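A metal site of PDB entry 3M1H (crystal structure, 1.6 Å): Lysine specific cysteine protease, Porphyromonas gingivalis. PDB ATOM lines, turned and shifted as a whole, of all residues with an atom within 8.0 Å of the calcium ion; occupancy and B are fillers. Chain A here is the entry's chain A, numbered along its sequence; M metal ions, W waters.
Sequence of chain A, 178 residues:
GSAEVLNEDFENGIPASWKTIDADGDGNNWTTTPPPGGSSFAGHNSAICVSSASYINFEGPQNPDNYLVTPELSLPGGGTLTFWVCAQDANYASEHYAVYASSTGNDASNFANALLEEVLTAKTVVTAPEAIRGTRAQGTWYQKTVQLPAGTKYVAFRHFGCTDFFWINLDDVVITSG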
ATOM      1  N   GLU A   8      20.711 -19.259   8.761  1.00  0.00           N
ATOM      2  CA  GLU A   8      21.644 -20.117   8.062  1.00  0.00           C
ATOM      3  C   GLU A   8      23.074 -19.564   8.067  1.00  0.00           C
ATOM      4  O   GLU A   8      23.356 -18.456   7.538  1.00  0.00           O
ATOM      5  CB  GLU A   8      21.192 -20.315   6.623  1.00  0.00           C
ATOM      6  CG  GLU A   8      22.029 -21.341   5.884  1.00  0.00           C
ATOM      7  CD  GLU A   8      22.197 -22.626   6.684  1.00  0.00           C
ATOM      8  OE1 GLU A   8      21.159 -23.172   7.105  1.00  0.00           O
ATOM      9  OE2 GLU A   8      23.342 -23.055   6.877  1.00  0.00           O
ATOM     10  N   ASP A   9      23.978 -20.366   8.625  1.00  0.00           N
ATOM     11  CA  ASP A   9      25.380 -20.002   8.777  1.00  0.00           C
ATOM     12  C   ASP A   9      26.276 -20.679   7.750  1.00  0.00           C
ATOM     13  O   ASP A   9      27.478 -20.442   7.740  1.00  0.00           O
ATOM     14  CB  ASP A   9      25.900 -20.248  10.226  1.00  0.00           C
ATOM     15  CG  ASP A   9      25.761 -21.695  10.673  1.00  0.00           C
ATOM     16  OD1 ASP A   9      25.641 -22.612   9.822  1.00  0.00           O
ATOM     17  OD2 ASP A   9      25.780 -21.879  11.929  1.00  0.00           O
ATOM     18  N   PHE A  10      25.712 -21.564   6.957  1.00  0.00           N
ATOM     19  CA  PHE A  10      26.411 -22.322   5.902  1.00  0.00           C
ATOM     20  C   PHE A  10      27.508 -23.258   6.392  1.00  0.00           C
ATOM     21  O   PHE A  10      28.274 -23.783   5.585  1.00  0.00           O
ATOM     22  CB  PHE A  10      26.895 -21.393   4.763  1.00  0.00           C
ATOM     23  CG  PHE A  10      25.758 -20.653   4.115  1.00  0.00           C
ATOM     24  CD1 PHE A  10      24.967 -21.272   3.163  1.00  0.00           C
ATOM     25  CD2 PHE A  10      25.458 -19.360   4.484  1.00  0.00           C
ATOM     26  CE1 PHE A  10      23.872 -20.644   2.571  1.00  0.00           C
ATOM     27  CE2 PHE A  10      24.357 -18.727   3.908  1.00  0.00           C
ATOM     28  CZ  PHE A  10      23.574 -19.355   2.962  1.00  0.00           C
ATOM     29  N   GLU A  11      27.572 -23.509   7.712  1.00  0.00           N
ATOM     30  CA  GLU A  11      28.673 -24.293   8.227  1.00  0.00           C
ATOM     31  C   GLU A  11      28.579 -25.773   7.832  1.00  0.00           C
ATOM     32  O   GLU A  11      29.611 -26.457   7.847  1.00  0.00           O
ATOM     33  CB  GLU A  11      28.785 -24.109   9.730  1.00  0.00           C
ATOM     34  CG  GLU A  11      29.112 -22.665  10.132  1.00  0.00           C
ATOM     35  CD  GLU A  11      30.399 -22.126   9.515  1.00  0.00           C
ATOM     36  OE1 GLU A  11      31.437 -22.820   9.522  1.00  0.00           O
ATOM     37  OE2 GLU A  11      30.396 -20.963   9.016  1.00  0.00           O
ATOM     38  N   ASN A  12      27.397 -26.224   7.449  1.00  0.00           N
ATOM     39  CA  ASN A  12      27.245 -27.521   6.789  1.00  0.00           C
ATOM     40  C   ASN A  12      27.028 -27.478   5.287  1.00  0.00           C
ATOM     41  O   ASN A  12      26.455 -28.401   4.690  1.00  0.00           O
ATOM     42  CB  ASN A  12      26.140 -28.296   7.500  1.00  0.00           C
ATOM     43  CG  ASN A  12      26.501 -28.540   8.946  1.00  0.00           C
ATOM     44  OD1 ASN A  12      27.522 -29.168   9.225  1.00  0.00           O
ATOM     45  ND2 ASN A  12      25.727 -27.990   9.846  1.00  0.00           N
ATOM     46  N   SER A  40      35.859 -23.565   1.188  1.00  0.00           N
ATOM     47  CA  SER A  40      35.275 -22.250   1.402  1.00  0.00           C
ATOM     48  C   SER A  40      36.307 -21.169   1.659  1.00  0.00           C
ATOM     49  O   SER A  40      37.342 -21.367   2.304  1.00  0.00           O
ATOM     50  CB  SER A  40      34.338 -22.316   2.602  1.00  0.00           C
ATOM     51  OG  SER A  40      33.662 -21.081   2.780  1.00  0.00           O
ATOM     52  N   PHE A  41      36.029 -19.994   1.135  1.00  0.00           N
ATOM     53  CA  PHE A  41      36.708 -18.780   1.565  1.00  0.00           C
ATOM     54  C   PHE A  41      36.340 -18.526   3.043  1.00  0.00           C
ATOM     55  O   PHE A  41      35.372 -19.072   3.566  1.00  0.00           O
ATOM     56  CB  PHE A  41      36.277 -17.597   0.695  1.00  0.00           C
ATOM     57  CG  PHE A  41      36.557 -17.755  -0.777  1.00  0.00           C
ATOM     58  CD1 PHE A  41      37.806 -18.136  -1.215  1.00  0.00           C
ATOM     59  CD2 PHE A  41      35.567 -17.510  -1.722  1.00  0.00           C
ATOM     60  CE1 PHE A  41      38.058 -18.312  -2.577  1.00  0.00           C
ATOM     61  CE2 PHE A  41      35.812 -17.655  -3.050  1.00  0.00           C
ATOM     62  CZ  PHE A  41      37.070 -18.051  -3.473  1.00  0.00           C
ATOM     63  N   ALA A  42      37.135 -17.720   3.710  1.00  0.00           N
ATOM     64  CA  ALA A  42      36.924 -17.428   5.122  1.00  0.00           C
ATOM     65  C   ALA A  42      35.557 -16.805   5.337  1.00  0.00           C
ATOM     66  O   ALA A  42      35.252 -15.800   4.688  1.00  0.00           O
ATOM     67  CB  ALA A  42      38.011 -16.506   5.649  1.00  0.00           C
ATOM     68  N   GLY A  43      34.729 -17.426   6.182  1.00  0.00           N
ATOM     69  CA  GLY A  43      33.366 -16.948   6.414  1.00  0.00           C
ATOM     70  C   GLY A  43      33.336 -15.751   7.342  1.00  0.00           C
ATOM     71  O   GLY A  43      34.363 -15.257   7.788  1.00  0.00           O
ATOM     72  N   HIS A  44      32.143 -15.263   7.625  1.00  0.00           N
ATOM     73  CA  HIS A  44      31.980 -14.130   8.502  1.00  0.00           C
ATOM     74  C   HIS A  44      32.105 -14.675   9.917  1.00  0.00           C
ATOM     75  O   HIS A  44      31.221 -15.420  10.396  1.00  0.00           O
ATOM     76  CB  HIS A  44      30.612 -13.485   8.248  1.00  0.00           C
ATOM     77  CG  HIS A  44      30.308 -12.389   9.217  1.00  0.00           C
ATOM     78  ND1 HIS A  44      29.200 -12.419  10.040  1.00  0.00           N
ATOM     79  CD2 HIS A  44      30.982 -11.262   9.521  1.00  0.00           C
ATOM     80  CE1 HIS A  44      29.213 -11.342  10.807  1.00  0.00           C
ATOM     81  NE2 HIS A  44      30.270 -10.617  10.506  1.00  0.00           N
ATOM     82  N   ASN A  45      33.207 -14.304  10.574  1.00  0.00           N
ATOM     83  CA  ASN A  45      33.527 -14.790  11.927  1.00  0.00           C
ATOM     84  C   ASN A  45      33.234 -16.279  12.040  1.00  0.00           C
ATOM     85  O   ASN A  45      32.695 -16.753  13.040  1.00  0.00           O
ATOM     86  CB  ASN A  45      32.701 -14.036  12.988  1.00  0.00           C
ATOM     87  CG  ASN A  45      33.033 -12.566  13.073  1.00  0.00           C
ATOM     88  OD1 ASN A  45      34.169 -12.165  12.846  1.00  0.00           O
ATOM     89  ND2 ASN A  45      32.041 -11.759  13.399  1.00  0.00           N
ATOM     90  N   SER A  46      33.560 -17.018  10.987  1.00  0.00           N
ATOM     91  CA  SER A  46      33.192 -18.416  10.879  1.00  0.00           C
ATOM     92  C   SER A  46      33.990 -19.056   9.715  1.00  0.00           C
ATOM     93  O   SER A  46      34.572 -18.347   8.889  1.00  0.00           O
ATOM     94  CB  SER A  46      31.690 -18.543  10.625  1.00  0.00           C
ATOM     95  OG  SER A  46      31.389 -18.061   9.319  1.00  0.00           O
ATOM     96  N   ALA A  47      33.985 -20.382   9.646  1.00  0.00           N
ATOM     97  CA  ALA A  47      34.759 -21.098   8.649  1.00  0.00           C
ATOM     98  C   ALA A  47      34.170 -21.043   7.230  1.00  0.00           C
ATOM     99  O   ALA A  47      34.929 -20.924   6.250  1.00  0.00           O
ATOM    100  CB  ALA A  47      34.962 -22.558   9.085  1.00  0.00           C
ATOM    101  N   ILE A  48      32.850 -21.134   7.108  1.00  0.00           N
ATOM    102  CA  ILE A  48      32.234 -21.308   5.781  1.00  0.00           C
ATOM    103  C   ILE A  48      31.323 -20.155   5.407  1.00  0.00           C
ATOM    104  O   ILE A  48      30.535 -19.676   6.217  1.00  0.00           O
ATOM    105  CB  ILE A  48      31.382 -22.597   5.687  1.00  0.00           C
ATOM    106  CG1 ILE A  48      32.119 -23.794   6.285  1.00  0.00           C
ATOM    107  CG2 ILE A  48      30.895 -22.834   4.232  1.00  0.00           C
ATOM    108  CD1 ILE A  48      33.402 -24.002   5.702  1.00  0.00           C
ATOM    109  N   CYS A  49      31.406 -19.754   4.140  1.00  0.00           N
ATOM    110  CA  CYS A  49      30.421 -18.905   3.528  1.00  0.00           C
ATOM    111  C   CYS A  49      30.123 -19.433   2.112  1.00  0.00           C
ATOM    112  O   CYS A  49      30.800 -20.360   1.627  1.00  0.00           O
ATOM    113  CB  CYS A  49      30.905 -17.458   3.489  1.00  0.00           C
ATOM    114  SG  CYS A  49      32.387 -17.178   2.477  1.00  0.00           S
ATOM    115  N   VAL A  50      29.095 -18.868   1.464  1.00  0.00           N
ATOM    116  CA  VAL A  50      28.677 -19.325   0.159  1.00  0.00           C
ATOM    117  C   VAL A  50      29.017 -18.220  -0.818  1.00  0.00           C
ATOM    118  O   VAL A  50      28.869 -17.045  -0.481  1.00  0.00           O
ATOM    119  CB  VAL A  50      27.193 -19.726   0.139  1.00  0.00           C
ATOM    120  CG1 VAL A  50      26.261 -18.527   0.418  1.00  0.00           C
ATOM    121  CG2 VAL A  50      26.848 -20.451  -1.163  1.00  0.00           C
ATOM    122  N   TRP A 141      33.206  -7.384   5.454  1.00  0.00           N
ATOM    123  CA  TRP A 141      31.858  -7.893   5.607  1.00  0.00           C
ATOM    124  C   TRP A 141      30.947  -6.754   6.042  1.00  0.00           C
ATOM    125  O   TRP A 141      31.216  -6.082   7.053  1.00  0.00           O
ATOM    126  CB  TRP A 141      31.779  -9.001   6.640  1.00  0.00           C
ATOM    127  CG  TRP A 141      32.407 -10.310   6.183  1.00  0.00           C
ATOM    128  CD1 TRP A 141      33.676 -10.763   6.462  1.00  0.00           C
ATOM    129  CD2 TRP A 141      31.777 -11.341   5.430  1.00  0.00           C
ATOM    130  NE1 TRP A 141      33.874 -12.004   5.904  1.00  0.00           N
ATOM    131  CE2 TRP A 141      32.721 -12.376   5.259  1.00  0.00           C
ATOM    132  CE3 TRP A 141      30.511 -11.475   4.843  1.00  0.00           C
ATOM    133  CZ2 TRP A 141      32.439 -13.534   4.536  1.00  0.00           C
ATOM    134  CZ3 TRP A 141      30.220 -12.642   4.138  1.00  0.00           C
ATOM    135  CH2 TRP A 141      31.198 -13.638   3.984  1.00  0.00           C
ATOM    136  N   LEU A 170      28.439 -14.558   0.736  1.00  0.00           N
ATOM    137  CA  LEU A 170      27.261 -14.349   1.559  1.00  0.00           C
ATOM    138  C   LEU A 170      27.379 -15.225   2.806  1.00  0.00           C
ATOM    139  O   LEU A 170      27.887 -16.360   2.709  1.00  0.00           O
ATOM    140  CB  LEU A 170      26.040 -14.737   0.725  1.00  0.00           C
ATOM    141  CG  LEU A 170      24.673 -14.798   1.381  1.00  0.00           C
ATOM    142  CD1 LEU A 170      24.176 -13.410   1.801  1.00  0.00           C
ATOM    143  CD2 LEU A 170      23.681 -15.492   0.428  1.00  0.00           C
ATOM    144  N   ASP A 171      26.903 -14.731   3.935  1.00  0.00           N
ATOM    145  CA  ASP A 171      26.908 -15.552   5.170  1.00  0.00           C
ATOM    146  C   ASP A 171      25.826 -15.035   6.109  1.00  0.00           C
ATOM    147  O   ASP A 171      25.302 -13.924   5.965  1.00  0.00           O
ATOM    148  CB  ASP A 171      28.298 -15.530   5.802  1.00  0.00           C
ATOM    149  CG  ASP A 171      28.613 -16.773   6.711  1.00  0.00           C
ATOM    150  OD1 ASP A 171      27.744 -17.612   6.886  1.00  0.00           O
ATOM    151  OD2 ASP A 171      29.796 -16.855   7.174  1.00  0.00           O
ATOM    152  N   ASP A 172      25.479 -15.870   7.099  1.00  0.00           N
ATOM    153  CA  ASP A 172      24.654 -15.458   8.231  1.00  0.00           C
ATOM    154  C   ASP A 172      23.325 -14.807   7.772  1.00  0.00           C
ATOM    155  O   ASP A 172      22.998 -13.667   8.115  1.00  0.00           O
ATOM    156  CB  ASP A 172      25.465 -14.579   9.176  1.00  0.00           C
ATOM    157  CG  ASP A 172      26.528 -15.353   9.945  1.00  0.00           C
ATOM    158  OD1 ASP A 172      26.331 -16.573  10.172  1.00  0.00           O
ATOM    159  OD2 ASP A 172      27.519 -14.750  10.371  1.00  0.00           O
ATOM    160  N   VAL A 173      22.565 -15.579   7.007  1.00  0.00           N
ATOM    161  CA  VAL A 173      21.237 -15.175   6.528  1.00  0.00           C
ATOM    162  C   VAL A 173      20.208 -15.454   7.605  1.00  0.00           C
ATOM    163  O   VAL A 173      20.043 -16.592   8.005  1.00  0.00           O
ATOM    164  CB  VAL A 173      20.875 -15.949   5.265  1.00  0.00           C
ATOM    165  CG1 VAL A 173      19.451 -15.587   4.789  1.00  0.00           C
ATOM    166  CG2 VAL A 173      21.892 -15.676   4.133  1.00  0.00           C
HETATM  167 CA    CA M   1      29.387 -19.049   8.118  1.00  0.00          CA
HETATM  168  O   HOH W   1      28.467 -18.208  10.133  1.00  0.00           O
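OD2 of Asp 171 lies close to N of His 44, 2.9 Å away.
The side-chain hydroxyl (OG) of Ser 46 sits close to the backbone carbonyl oxygen (O) of His 44.
Five residues have an atom within 4 Å of the calcium ion: Asp 9, Glu 11, Ser 46, Ile 48 and Asp 171.
The nearest printed residue that does not touch the calcium ion is Asp 172 (4.4 Å).
The calcium ion is bound by the backbone carbonyl oxygen (O) of Ile 48, the side-chain carboxylate (OE2) of Glu 11, water W1, the backbone carbonyl oxygen (O) of Asp 9, the side-chain carboxylate (OD2) of Asp 171, the side-chain carboxylate (OD1) of Asp 171 and the side-chain hydroxyl (OG) of Ser 46.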
